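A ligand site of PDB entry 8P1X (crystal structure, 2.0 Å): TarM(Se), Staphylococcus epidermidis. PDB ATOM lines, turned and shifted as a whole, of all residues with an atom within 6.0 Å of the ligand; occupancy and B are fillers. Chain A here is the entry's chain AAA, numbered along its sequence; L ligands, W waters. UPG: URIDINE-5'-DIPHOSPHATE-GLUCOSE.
The backbone NH (N) of Ser 424 is in hydrogen-bond range of an oxygen (O1A) of the ligand. N of Thr 399 lies within hydrogen-bond range of O4 of the ligand (3.0 Å). OG1 of Thr 36 is in hydrogen-bond range of O3C of the ligand (3.4 Å). O2' of the ligand is in hydrogen-bond range of NE2 of Gln 346 (3.2 Å). The side-chain amide nitrogen (ND2) of Asn 320 is in hydrogen-bond range of an oxygen (O6') of the ligand (2.7 Å). The guanidinium group (NH1) of Arg 342 is in salt-bridge range of an oxygen (O2B) of the ligand (2.8 Å). The backbone NH (N) of Met 34 lies within hydrogen-bond range of an oxygen (O5') of the ligand (3.5 Å). The side-chain carboxylate (OE2) of Glu 427 is in hydrogen-bond range of an oxygen (O3C) of the ligand, 2.6 Å away. An oxygen (O4') of the ligand sits at hydrogen-bond distance from the backbone carbonyl oxygen (O) of Gln 421 (2.5 Å). N of Gln 421 lies within hydrogen-bond range of O3' of the ligand (2.8 Å). An oxygen (O3') of the ligand is in hydrogen-bond range of the backbone NH of Gly 420, at 2.7 Å. O2A of the ligand lies close to N of Leu 423, 3.2 Å away. The side-chain amino group (NZ) of Lys 347 is in salt-bridge range of an oxygen (O2B) of the ligand (3.0 Å). ND1 of His 265 lies within hydrogen-bond range of O6' of the ligand, 2.9 Å away. A nitrogen (N3) of the ligand lies within hydrogen-bond range of the backbone carbonyl oxygen (O) of Thr 399 (2.9 Å). O1B of the ligand sits at hydrogen-bond distance from N of Gly 33, at 2.8 Å. The side-chain hydroxyl (OG) of Ser 424 sits at hydrogen-bond distance from an oxygen (O1A) of the ligand. An oxygen (O3') of the ligand sits at hydrogen-bond distance from the side-chain carboxylate (OE1) of Glu 419 (2.8 Å). An oxygen (O2) of the ligand sits at hydrogen-bond distance from the side-chain hydroxyl (OH) of Tyr 398, 3.4 Å away.
The side-chain hydroxyl of Thr 36 sits at hydrogen-bond distance from the backbone carbonyl oxygen of Gly 32, at 3.2 Å. OG1 of Thr 399 sits at hydrogen-bond distance from N of Asn 401 (3.0 Å). NZ of Lys 347 lies within salt-bridge range of OE2 of Glu 419 (2.8 Å). ND2 of Asn 320 lies close to NE2 of Gln 421 (3.2 Å). OG of Ser 424 is in hydrogen-bond range of O of Ile 340, at 2.9 Å. The backbone NH (N) of Gly 420 sits close to the backbone carbonyl oxygen (O) of Tyr 442 (3.3 Å). NH1 of Arg 342 sits at hydrogen-bond distance from OE1 of Gln 346 (3.2 Å). The backbone carbonyl oxygen (O) of Lys 31 sits at hydrogen-bond distance from the side-chain hydroxyl (OH) of Tyr 398 (2.7 Å).
Lys 31 touches the ligand. CA of Gly 32 touches O4C of the ligand, 3.4 Å away. Ala 37 touches the ligand (CB to C6', 3.96 Å). Val 266 touches the ligand. CD1 of Leu 298 touches O6' of the ligand, 3.4 Å away. Ile 340 touches the ligand (CG2 to C5, 3.4 Å). Ser 341 touches the ligand (N to C5, 3.7 Å). C of Tyr 371 touches O4 of the ligand, 3.9 Å away. Gly 372 touches the ligand. Ala 402 touches the ligand (CB to O2C, 3.99 Å). Of the 36 residues printed, 26 come within 4 Å of the ligand.
Water W4 lies within hydrogen-bond range of O1A of the ligand and NZ of Lys 347. Water W1 bridges an oxygen (O1B) of the ligand (2.9 Å) and the backbone NH (N) of Arg 342 (3.1 Å). Water W2 lies within hydrogen-bond range of an oxygen (O1A) of the ligand (3.0 Å), the backbone NH of Leu 425 (3.3 Å) and the backbone NH of Ser 424 (3.4 Å). Water W5 lies within hydrogen-bond range of the backbone NH of Met 34 (3.1 Å), the backbone NH of Gly 33 (3.2 Å) and an oxygen (O1B) of the ligand (3.3 Å).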
ATOM      1  N   LYS A  31       0.651  24.347  -1.424  1.00  0.00           N
ATOM      2  CA  LYS A  31       2.105  24.374  -1.111  1.00  0.00           C
ATOM      3  C   LYS A  31       2.411  25.407  -0.022  1.00  0.00           C
ATOM      4  O   LYS A  31       1.484  26.128   0.401  1.00  0.00           O
ATOM      5  CB  LYS A  31       2.922  24.580  -2.391  1.00  0.00           C
ATOM      6  CG  LYS A  31       3.690  23.338  -2.851  1.00  0.00           C
ATOM      7  CD  LYS A  31       2.827  22.297  -3.528  1.00  0.00           C
ATOM      8  N   GLY A  32       3.665  25.435   0.422  1.00  0.00           N
ATOM      9  CA  GLY A  32       4.115  26.204   1.607  1.00  0.00           C
ATOM     10  C   GLY A  32       4.872  27.462   1.226  1.00  0.00           C
ATOM     11  O   GLY A  32       4.516  28.103   0.204  1.00  0.00           O
ATOM     12  N   GLY A  33       5.873  27.818   2.022  1.00  0.00           N
ATOM     13  CA  GLY A  33       6.586  29.105   1.953  1.00  0.00           C
ATOM     14  C   GLY A  33       7.351  29.310   0.659  1.00  0.00           C
ATOM     15  O   GLY A  33       7.360  30.441   0.160  1.00  0.00           O
ATOM     16  N   MET A  34       8.012  28.272   0.127  1.00  0.00           N
ATOM     17  CA  MET A  34       8.893  28.445  -1.054  1.00  0.00           C
ATOM     18  C   MET A  34       8.059  28.947  -2.238  1.00  0.00           C
ATOM     19  O   MET A  34       8.483  29.927  -2.869  1.00  0.00           O
ATOM     20  CB  MET A  34       9.606  27.147  -1.454  1.00  0.00           C
ATOM     21  CG  MET A  34      10.641  27.384  -2.540  1.00  0.00           C
ATOM     22  SD  MET A  34      11.554  25.900  -2.987  1.00  0.00           S
ATOM     23  CE  MET A  34      12.105  25.331  -1.382  1.00  0.00           C
ATOM     24  N   THR A  36       5.098  30.409  -2.203  1.00  0.00           N
ATOM     25  CA  THR A  36       4.605  31.767  -1.836  1.00  0.00           C
ATOM     26  C   THR A  36       5.719  32.778  -2.131  1.00  0.00           C
ATOM     27  O   THR A  36       5.433  33.778  -2.815  1.00  0.00           O
ATOM     28  CB  THR A  36       4.127  31.849  -0.385  1.00  0.00           C
ATOM     29  OG1 THR A  36       3.043  30.941  -0.223  1.00  0.00           O
ATOM     30  CG2 THR A  36       3.672  33.230   0.014  1.00  0.00           C
ATOM     31  N   ALA A  37       6.941  32.530  -1.647  1.00  0.00           N
ATOM     32  CA  ALA A  37       8.098  33.436  -1.802  1.00  0.00           C
ATOM     33  C   ALA A  37       8.339  33.715  -3.287  1.00  0.00           C
ATOM     34  O   ALA A  37       8.401  34.905  -3.660  1.00  0.00           O
ATOM     35  CB  ALA A  37       9.321  32.848  -1.143  1.00  0.00           C
ATOM     36  N   LYS A  75      -2.732  34.481  -5.481  1.00  0.00           N
ATOM     37  CA  LYS A  75      -1.394  34.007  -5.065  1.00  0.00           C
ATOM     38  C   LYS A  75      -0.381  34.324  -6.179  1.00  0.00           C
ATOM     39  O   LYS A  75       0.757  34.663  -5.855  1.00  0.00           O
ATOM     40  CB  LYS A  75      -1.434  32.526  -4.699  1.00  0.00           C
ATOM     41  CG  LYS A  75      -2.487  32.148  -3.667  1.00  0.00           C
ATOM     42  CD  LYS A  75      -2.555  33.086  -2.474  1.00  0.00           C
ATOM     43  CE  LYS A  75      -3.509  32.609  -1.397  1.00  0.00           C
ATOM     44  N   ILE A 264      18.658  29.832  -0.711  1.00  0.00           N
ATOM     45  CA  ILE A 264      18.487  28.886   0.417  1.00  0.00           C
ATOM     46  C   ILE A 264      17.271  29.353   1.222  1.00  0.00           C
ATOM     47  O   ILE A 264      17.340  30.451   1.806  1.00  0.00           O
ATOM     48  CB  ILE A 264      19.768  28.799   1.268  1.00  0.00           C
ATOM     49  CG1 ILE A 264      21.002  28.497   0.398  1.00  0.00           C
ATOM     50  CG2 ILE A 264      19.611  27.797   2.391  1.00  0.00           C
ATOM     51  CD1 ILE A 264      20.929  27.177  -0.347  1.00  0.00           C
ATOM     52  N   HIS A 265      16.203  28.554   1.222  1.00  0.00           N
ATOM     53  CA  HIS A 265      14.915  28.907   1.868  1.00  0.00           C
ATOM     54  C   HIS A 265      14.842  28.363   3.284  1.00  0.00           C
ATOM     55  O   HIS A 265      13.879  28.706   3.974  1.00  0.00           O
ATOM     56  CB  HIS A 265      13.751  28.374   1.024  1.00  0.00           C
ATOM     57  CG  HIS A 265      13.599  29.095  -0.271  1.00  0.00           C
ATOM     58  ND1 HIS A 265      12.811  30.222  -0.401  1.00  0.00           N
ATOM     59  CD2 HIS A 265      14.130  28.852  -1.487  1.00  0.00           C
ATOM     60  CE1 HIS A 265      12.845  30.631  -1.643  1.00  0.00           C
ATOM     61  NE2 HIS A 265      13.650  29.811  -2.327  1.00  0.00           N
ATOM     62  N   VAL A 266      15.790  27.513   3.702  1.00  0.00           N
ATOM     63  CA  VAL A 266      15.658  26.770   4.995  1.00  0.00           C
ATOM     64  C   VAL A 266      17.033  26.558   5.631  1.00  0.00           C
ATOM     65  O   VAL A 266      18.046  26.579   4.906  1.00  0.00           O
ATOM     66  CB  VAL A 266      14.911  25.440   4.785  1.00  0.00           C
ATOM     67  CG1 VAL A 266      15.810  24.352   4.204  1.00  0.00           C
ATOM     68  CG2 VAL A 266      14.259  24.952   6.071  1.00  0.00           C
ATOM     69  N   LEU A 298      18.374  34.231   3.532  1.00  0.00           N
ATOM     70  CA  LEU A 298      17.273  35.085   4.047  1.00  0.00           C
ATOM     71  C   LEU A 298      17.719  35.842   5.298  1.00  0.00           C
ATOM     72  O   LEU A 298      17.078  36.841   5.614  1.00  0.00           O
ATOM     73  CB  LEU A 298      16.061  34.213   4.311  1.00  0.00           C
ATOM     74  CG  LEU A 298      15.597  33.340   3.144  1.00  0.00           C
ATOM     75  CD1 LEU A 298      14.506  32.390   3.586  1.00  0.00           C
ATOM     76  CD2 LEU A 298      15.117  34.197   1.976  1.00  0.00           C
ATOM     77  N   ASN A 320      12.924  37.538   1.902  1.00  0.00           N
ATOM     78  CA  ASN A 320      11.758  37.287   1.017  1.00  0.00           C
ATOM     79  C   ASN A 320      10.959  38.585   0.907  1.00  0.00           C
ATOM     80  O   ASN A 320      10.851  39.282   1.920  1.00  0.00           O
ATOM     81  CB  ASN A 320      10.869  36.170   1.559  1.00  0.00           C
ATOM     82  CG  ASN A 320      11.474  34.799   1.330  1.00  0.00           C
ATOM     83  OD1 ASN A 320      11.934  34.491   0.234  1.00  0.00           O
ATOM     84  ND2 ASN A 320      11.445  33.969   2.358  1.00  0.00           N
ATOM     85  N   ILE A 340      -0.703  27.720  11.105  1.00  0.00           N
ATOM     86  CA  ILE A 340      -0.897  27.439   9.655  1.00  0.00           C
ATOM     87  C   ILE A 340       0.456  27.003   9.073  1.00  0.00           C
ATOM     88  O   ILE A 340       1.365  27.844   9.003  1.00  0.00           O
ATOM     89  CB  ILE A 340      -1.464  28.689   8.957  1.00  0.00           C
ATOM     90  CG1 ILE A 340      -2.848  29.038   9.511  1.00  0.00           C
ATOM     91  CG2 ILE A 340      -1.482  28.517   7.444  1.00  0.00           C
ATOM     92  CD1 ILE A 340      -3.444  30.302   8.940  1.00  0.00           C
ATOM     93  N   SER A 341       0.581  25.743   8.669  1.00  0.00           N
ATOM     94  CA  SER A 341       1.865  25.151   8.194  1.00  0.00           C
ATOM     95  C   SER A 341       1.633  23.846   7.432  1.00  0.00           C
ATOM     96  O   SER A 341       0.564  23.243   7.577  1.00  0.00           O
ATOM     97  CB  SER A 341       2.778  24.902   9.347  1.00  0.00           C
ATOM     98  OG  SER A 341       2.473  23.652   9.954  1.00  0.00           O
ATOM     99  N   ARG A 342       2.650  23.407   6.701  1.00  0.00           N
ATOM    100  CA  ARG A 342       2.735  22.004   6.221  1.00  0.00           C
ATOM    101  C   ARG A 342       2.852  21.127   7.480  1.00  0.00           C
ATOM    102  O   ARG A 342       3.598  21.533   8.390  1.00  0.00           O
ATOM    103  CB  ARG A 342       3.925  21.819   5.281  1.00  0.00           C
ATOM    104  CG  ARG A 342       3.944  22.783   4.100  1.00  0.00           C
ATOM    105  CD  ARG A 342       5.215  22.666   3.262  1.00  0.00           C
ATOM    106  NE  ARG A 342       6.384  23.231   3.942  1.00  0.00           N
ATOM    107  CZ  ARG A 342       7.427  22.547   4.403  1.00  0.00           C
ATOM    108  NH1 ARG A 342       8.409  23.184   5.013  1.00  0.00           N
ATOM    109  NH2 ARG A 342       7.514  21.237   4.244  1.00  0.00           N
ATOM    110  N   GLN A 346       9.493  19.248  10.924  1.00  0.00           N
ATOM    111  CA  GLN A 346      10.109  20.594  11.088  1.00  0.00           C
ATOM    112  C   GLN A 346       9.283  21.463  12.045  1.00  0.00           C
ATOM    113  O   GLN A 346       9.889  22.198  12.840  1.00  0.00           O
ATOM    114  CB  GLN A 346      10.265  21.272   9.720  1.00  0.00           C
ATOM    115  CG  GLN A 346      10.452  22.787   9.800  1.00  0.00           C
ATOM    116  CD  GLN A 346      10.618  23.425   8.439  1.00  0.00           C
ATOM    117  OE1 GLN A 346      10.477  22.769   7.398  1.00  0.00           O
ATOM    118  NE2 GLN A 346      10.921  24.709   8.421  1.00  0.00           N
ATOM    119  N   LYS A 347       7.955  21.391  11.968  1.00  0.00           N
ATOM    120  CA  LYS A 347       7.028  22.359  12.620  1.00  0.00           C
ATOM    121  C   LYS A 347       6.821  22.031  14.114  1.00  0.00           C
ATOM    122  O   LYS A 347       6.172  22.850  14.813  1.00  0.00           O
ATOM    123  CB  LYS A 347       5.725  22.419  11.817  1.00  0.00           C
ATOM    124  CG  LYS A 347       5.907  22.899  10.383  1.00  0.00           C
ATOM    125  CD  LYS A 347       6.639  24.224  10.250  1.00  0.00           C
ATOM    126  CE  LYS A 347       6.850  24.629   8.807  1.00  0.00           C
ATOM    127  NZ  LYS A 347       7.535  25.938   8.698  1.00  0.00           N
ATOM    128  N   TYR A 371      -4.108  24.534  10.697  1.00  0.00           N
ATOM    129  CA  TYR A 371      -4.412  24.483   9.242  1.00  0.00           C
ATOM    130  C   TYR A 371      -3.198  23.916   8.505  1.00  0.00           C
ATOM    131  O   TYR A 371      -2.059  24.326   8.803  1.00  0.00           O
ATOM    132  CB  TYR A 371      -4.768  25.867   8.700  1.00  0.00           C
ATOM    133  CG  TYR A 371      -6.172  26.335   9.032  1.00  0.00           C
ATOM    134  CD1 TYR A 371      -7.242  26.002   8.218  1.00  0.00           C
ATOM    135  CD2 TYR A 371      -6.419  27.110  10.154  1.00  0.00           C
ATOM    136  CE1 TYR A 371      -8.524  26.428   8.506  1.00  0.00           C
ATOM    137  CE2 TYR A 371      -7.699  27.533  10.464  1.00  0.00           C
ATOM    138  CZ  TYR A 371      -8.759  27.200   9.636  1.00  0.00           C
ATOM    139  OH  TYR A 371     -10.018  27.618   9.926  1.00  0.00           O
ATOM    140  N   GLY A 372      -3.450  22.986   7.584  1.00  0.00           N
ATOM    141  CA  GLY A 372      -2.410  22.464   6.681  1.00  0.00           C
ATOM    142  C   GLY A 372      -2.572  20.977   6.432  1.00  0.00           C
ATOM    143  O   GLY A 372      -3.390  20.338   7.099  1.00  0.00           O
ATOM    144  N   THR A 373      -1.813  20.452   5.466  1.00  0.00           N
ATOM    145  CA  THR A 373      -1.796  19.017   5.114  1.00  0.00           C
ATOM    146  C   THR A 373      -0.368  18.500   5.236  1.00  0.00           C
ATOM    147  O   THR A 373       0.565  19.312   5.091  1.00  0.00           O
ATOM    148  CB  THR A 373      -2.312  18.788   3.684  1.00  0.00           C
ATOM    149  OG1 THR A 373      -1.480  19.535   2.804  1.00  0.00           O
ATOM    150  CG2 THR A 373      -3.760  19.210   3.515  1.00  0.00           C
ATOM    151  N   GLY A 397      -7.353  21.116   7.823  1.00  0.00           N
ATOM    152  CA  GLY A 397      -6.908  20.931   6.433  1.00  0.00           C
ATOM    153  C   GLY A 397      -6.306  22.195   5.844  1.00  0.00           C
ATOM    154  O   GLY A 397      -6.132  23.191   6.581  1.00  0.00           O
ATOM    155  N   TYR A 398      -5.967  22.163   4.556  1.00  0.00           N
ATOM    156  CA  TYR A 398      -5.272  23.285   3.863  1.00  0.00           C
ATOM    157  C   TYR A 398      -6.270  24.403   3.613  1.00  0.00           C
ATOM    158  O   TYR A 398      -7.439  24.112   3.316  1.00  0.00           O
ATOM    159  CB  TYR A 398      -4.618  22.821   2.556  1.00  0.00           C
ATOM    160  CG  TYR A 398      -3.690  23.855   1.949  1.00  0.00           C
ATOM    161  CD1 TYR A 398      -4.185  24.831   1.098  1.00  0.00           C
ATOM    162  CD2 TYR A 398      -2.334  23.851   2.225  1.00  0.00           C
ATOM    163  CE1 TYR A 398      -3.348  25.781   0.527  1.00  0.00           C
ATOM    164  CE2 TYR A 398      -1.483  24.790   1.656  1.00  0.00           C
ATOM    165  CZ  TYR A 398      -1.997  25.761   0.807  1.00  0.00           C
ATOM    166  OH  TYR A 398      -1.176  26.692   0.239  1.00  0.00           O
ATOM    167  N   THR A 399      -5.837  25.650   3.738  1.00  0.00           N
ATOM    168  CA  THR A 399      -6.669  26.840   3.440  1.00  0.00           C
ATOM    169  C   THR A 399      -5.960  27.671   2.373  1.00  0.00           C
ATOM    170  O   THR A 399      -4.771  27.983   2.545  1.00  0.00           O
ATOM    171  CB  THR A 399      -7.032  27.613   4.720  1.00  0.00           C
ATOM    172  OG1 THR A 399      -7.812  28.740   4.317  1.00  0.00           O
ATOM    173  CG2 THR A 399      -5.838  28.066   5.527  1.00  0.00           C
ATOM    174  N   THR A 400      -6.665  28.011   1.297  1.00  0.00           N
ATOM    175  CA  THR A 400      -6.192  28.964   0.267  1.00  0.00           C
ATOM    176  C   THR A 400      -6.504  30.371   0.776  1.00  0.00           C
ATOM    177  O   THR A 400      -6.131  31.337   0.097  1.00  0.00           O
ATOM    178  CB  THR A 400      -6.826  28.643  -1.089  1.00  0.00           C
ATOM    179  OG1 THR A 400      -8.241  28.638  -0.904  1.00  0.00           O
ATOM    180  CG2 THR A 400      -6.369  27.308  -1.654  1.00  0.00           C
ATOM    181  N   ASN A 401      -7.186  30.467   1.925  1.00  0.00           N
ATOM    182  CA  ASN A 401      -7.636  31.745   2.535  1.00  0.00           C
ATOM    183  C   ASN A 401      -7.088  31.847   3.959  1.00  0.00           C
ATOM    184  O   ASN A 401      -7.903  31.857   4.907  1.00  0.00           O
ATOM    185  CB  ASN A 401      -9.162  31.850   2.500  1.00  0.00           C
ATOM    186  N   ALA A 402      -5.765  31.907   4.102  1.00  0.00           N
ATOM    187  CA  ALA A 402      -5.060  31.975   5.394  1.00  0.00           C
ATOM    188  C   ALA A 402      -5.382  33.297   6.105  1.00  0.00           C
ATOM    189  O   ALA A 402      -5.587  33.278   7.329  1.00  0.00           O
ATOM    190  CB  ALA A 402      -3.577  31.829   5.178  1.00  0.00           C
ATOM    191  N   PHE A 418      13.190  24.414  13.067  1.00  0.00           N
ATOM    192  CA  PHE A 418      14.087  25.139  12.133  1.00  0.00           C
ATOM    193  C   PHE A 418      13.284  25.908  11.076  1.00  0.00           C
ATOM    194  O   PHE A 418      12.149  25.515  10.739  1.00  0.00           O
ATOM    195  CB  PHE A 418      15.115  24.187  11.507  1.00  0.00           C
ATOM    196  CG  PHE A 418      14.567  23.026  10.728  1.00  0.00           C
ATOM    197  CD1 PHE A 418      14.331  23.127   9.362  1.00  0.00           C
ATOM    198  CD2 PHE A 418      14.337  21.804  11.337  1.00  0.00           C
ATOM    199  CE1 PHE A 418      13.835  22.055   8.632  1.00  0.00           C
ATOM    200  CE2 PHE A 418      13.832  20.730  10.608  1.00  0.00           C
ATOM    201  CZ  PHE A 418      13.591  20.855   9.259  1.00  0.00           C
ATOM    202  N   GLU A 419      13.874  26.991  10.576  1.00  0.00           N
ATOM    203  CA  GLU A 419      13.252  27.865   9.549  1.00  0.00           C
ATOM    204  C   GLU A 419      14.353  28.494   8.689  1.00  0.00           C
ATOM    205  O   GLU A 419      15.528  28.366   9.045  1.00  0.00           O
ATOM    206  CB  GLU A 419      12.426  28.967  10.221  1.00  0.00           C
ATOM    207  CG  GLU A 419      11.169  28.476  10.914  1.00  0.00           C
ATOM    208  CD  GLU A 419      10.041  28.029   9.998  1.00  0.00           C
ATOM    209  OE1 GLU A 419      10.023  28.450   8.826  1.00  0.00           O
ATOM    210  OE2 GLU A 419       9.173  27.263  10.479  1.00  0.00           O
ATOM    211  N   GLY A 420      13.974  29.128   7.582  1.00  0.00           N
ATOM    212  CA  GLY A 420      14.810  30.097   6.864  1.00  0.00           C
ATOM    213  C   GLY A 420      14.367  31.500   7.202  1.00  0.00           C
ATOM    214  O   GLY A 420      15.215  32.401   7.272  1.00  0.00           O
ATOM    215  N   GLN A 421      13.046  31.653   7.388  1.00  0.00           N
ATOM    216  CA  GLN A 421      12.348  32.892   7.805  1.00  0.00           C
ATOM    217  C   GLN A 421      10.895  32.490   8.110  1.00  0.00           C
ATOM    218  O   GLN A 421      10.370  31.652   7.361  1.00  0.00           O
ATOM    219  CB  GLN A 421      12.427  33.918   6.678  1.00  0.00           C
ATOM    220  CG  GLN A 421      12.229  35.353   7.132  1.00  0.00           C
ATOM    221  CD  GLN A 421      12.280  36.321   5.972  1.00  0.00           C
ATOM    222  OE1 GLN A 421      12.177  37.534   6.155  1.00  0.00           O
ATOM    223  NE2 GLN A 421      12.449  35.792   4.764  1.00  0.00           N
ATOM    224  N   GLY A 422      10.286  33.011   9.162  1.00  0.00           N
ATOM    225  CA  GLY A 422       8.910  32.601   9.518  1.00  0.00           C
ATOM    226  C   GLY A 422       7.867  33.340   8.689  1.00  0.00           C
ATOM    227  O   GLY A 422       7.382  34.364   9.172  1.00  0.00           O
ATOM    228  N   LEU A 423       7.494  32.836   7.507  1.00  0.00           N
ATOM    229  CA  LEU A 423       6.517  33.553   6.624  1.00  0.00           C
ATOM    230  C   LEU A 423       5.118  33.527   7.258  1.00  0.00           C
ATOM    231  O   LEU A 423       4.433  34.544   7.190  1.00  0.00           O
ATOM    232  CB  LEU A 423       6.508  32.958   5.214  1.00  0.00           C
ATOM    233  CG  LEU A 423       6.947  33.910   4.106  1.00  0.00           C
ATOM    234  CD1 LEU A 423       8.281  34.574   4.423  1.00  0.00           C
ATOM    235  CD2 LEU A 423       7.025  33.188   2.775  1.00  0.00           C
ATOM    236  N   SER A 424       4.718  32.408   7.864  1.00  0.00           N
ATOM    237  CA  SER A 424       3.419  32.288   8.571  1.00  0.00           C
ATOM    238  C   SER A 424       3.411  33.238   9.783  1.00  0.00           C
ATOM    239  O   SER A 424       2.363  33.870  10.014  1.00  0.00           O
ATOM    240  CB  SER A 424       3.137  30.865   8.957  1.00  0.00           C
ATOM    241  OG  SER A 424       2.613  30.156   7.841  1.00  0.00           O
ATOM    242  N   LEU A 425       4.532  33.352  10.499  1.00  0.00           N
ATOM    243  CA  LEU A 425       4.679  34.286  11.642  1.00  0.00           C
ATOM    244  C   LEU A 425       4.538  35.721  11.112  1.00  0.00           C
ATOM    245  O   LEU A 425       3.799  36.508  11.723  1.00  0.00           O
ATOM    246  CB  LEU A 425       6.035  34.079  12.334  1.00  0.00           C
ATOM    247  CG  LEU A 425       6.161  32.803  13.160  1.00  0.00           C
ATOM    248  CD1 LEU A 425       7.616  32.496  13.467  1.00  0.00           C
ATOM    249  CD2 LEU A 425       5.349  32.902  14.437  1.00  0.00           C
ATOM    250  N   GLU A 427       3.098  36.762   8.314  1.00  0.00           N
ATOM    251  CA  GLU A 427       1.704  36.912   7.826  1.00  0.00           C
ATOM    252  C   GLU A 427       0.801  37.274   9.007  1.00  0.00           C
ATOM    253  O   GLU A 427      -0.012  38.215   8.867  1.00  0.00           O
ATOM    254  CB  GLU A 427       1.227  35.647   7.108  1.00  0.00           C
ATOM    255  CG  GLU A 427       1.747  35.528   5.685  1.00  0.00           C
ATOM    256  CD  GLU A 427       1.677  34.142   5.066  1.00  0.00           C
ATOM    257  OE1 GLU A 427       0.891  33.302   5.552  1.00  0.00           O
ATOM    258  OE2 GLU A 427       2.423  33.909   4.092  1.00  0.00           O
ATOM    259  N   TYR A 442      18.039  30.724  12.085  1.00  0.00           N
ATOM    260  CA  TYR A 442      17.643  31.396  10.835  1.00  0.00           C
ATOM    261  C   TYR A 442      16.123  31.485  10.824  1.00  0.00           C
ATOM    262  O   TYR A 442      15.474  31.054   9.875  1.00  0.00           O
ATOM    263  CB  TYR A 442      18.214  30.633   9.638  1.00  0.00           C
ATOM    264  CG  TYR A 442      19.510  29.930   9.908  1.00  0.00           C
ATOM    265  CD1 TYR A 442      20.517  30.536  10.639  1.00  0.00           C
ATOM    266  CD2 TYR A 442      19.746  28.660   9.411  1.00  0.00           C
ATOM    267  CE1 TYR A 442      21.711  29.905  10.881  1.00  0.00           C
ATOM    268  CE2 TYR A 442      20.946  28.006   9.636  1.00  0.00           C
ATOM    269  CZ  TYR A 442      21.936  28.636  10.363  1.00  0.00           C
ATOM    270  OH  TYR A 442      23.120  28.000  10.592  1.00  0.00           O
HETATM  271  N1  UPG L   1       0.008  27.928   3.939  1.00  0.00           N
HETATM  272  C2  UPG L   1      -1.256  28.179   3.454  1.00  0.00           C
HETATM  273  N3  UPG L   1      -2.237  27.321   3.873  1.00  0.00           N
HETATM  274  C4  UPG L   1      -2.081  26.259   4.739  1.00  0.00           C
HETATM  275  C5  UPG L   1      -0.748  26.062   5.222  1.00  0.00           C
HETATM  276  C6  UPG L   1       0.230  26.894   4.822  1.00  0.00           C
HETATM  277  O2  UPG L   1      -1.486  29.104   2.683  1.00  0.00           O
HETATM  278  O4  UPG L   1      -3.072  25.575   5.020  1.00  0.00           O
HETATM  279  C1C UPG L   1       1.074  28.864   3.542  1.00  0.00           C
HETATM  280  C2C UPG L   1       1.166  30.062   4.495  1.00  0.00           C
HETATM  281  O2C UPG L   1       0.202  31.037   4.177  1.00  0.00           O
HETATM  282  C3C UPG L   1       2.589  30.550   4.219  1.00  0.00           C
HETATM  283  C4C UPG L   1       3.340  29.241   3.914  1.00  0.00           C
HETATM  284  O4C UPG L   1       2.332  28.235   3.612  1.00  0.00           O
HETATM  285  O3C UPG L   1       2.675  31.475   3.145  1.00  0.00           O
HETATM  286  C5C UPG L   1       4.215  28.731   5.034  1.00  0.00           C
HETATM  287  O5C UPG L   1       5.503  29.374   4.917  1.00  0.00           O
HETATM  288  PA  UPG L   1       6.527  29.353   6.152  1.00  0.00           P
HETATM  289  O1A UPG L   1       5.804  29.672   7.413  1.00  0.00           O
HETATM  290  O2A UPG L   1       7.705  30.174   5.775  1.00  0.00           O
HETATM  291  O3A UPG L   1       6.962  27.802   6.171  1.00  0.00           O
HETATM  292  PB  UPG L   1       7.633  26.794   5.117  1.00  0.00           P
HETATM  293  O1B UPG L   1       6.564  26.241   4.227  1.00  0.00           O
HETATM  294  O2B UPG L   1       8.439  25.797   5.885  1.00  0.00           O
HETATM  295  O3B UPG L   1       8.605  27.772   4.290  1.00  0.00           O
HETATM  296  C1' UPG L   1       9.920  27.514   3.850  1.00  0.00           C
HETATM  297  C2' UPG L   1      10.887  27.744   4.998  1.00  0.00           C
HETATM  298  C3' UPG L   1      10.642  29.137   5.531  1.00  0.00           C
HETATM  299  C4' UPG L   1      10.857  30.158   4.433  1.00  0.00           C
HETATM  300  C5' UPG L   1      10.030  29.806   3.184  1.00  0.00           C
HETATM  301  C6' UPG L   1      10.365  30.664   1.985  1.00  0.00           C
HETATM  302  O2' UPG L   1      10.755  26.744   6.006  1.00  0.00           O
HETATM  303  O3' UPG L   1      11.486  29.397   6.653  1.00  0.00           O
HETATM  304  O4' UPG L   1      10.450  31.441   4.878  1.00  0.00           O
HETATM  305  O5' UPG L   1      10.241  28.417   2.808  1.00  0.00           O
HETATM  306  O6' UPG L   1      11.645  31.255   2.093  1.00  0.00           O
HETATM  307  O   HOH W   1       4.659  25.714   6.328  1.00  0.00           O
HETATM  308  O   HOH W   2       6.455  30.719  10.192  1.00  0.00           O
HETATM  309  O   HOH W   3      -1.130  32.116   2.119  1.00  0.00           O
HETATM  310  O   HOH W   4       5.004  27.441   8.875  1.00  0.00           O
HETATM  311  O   HOH W   5       7.830  25.374   1.259  1.00  0.00           O
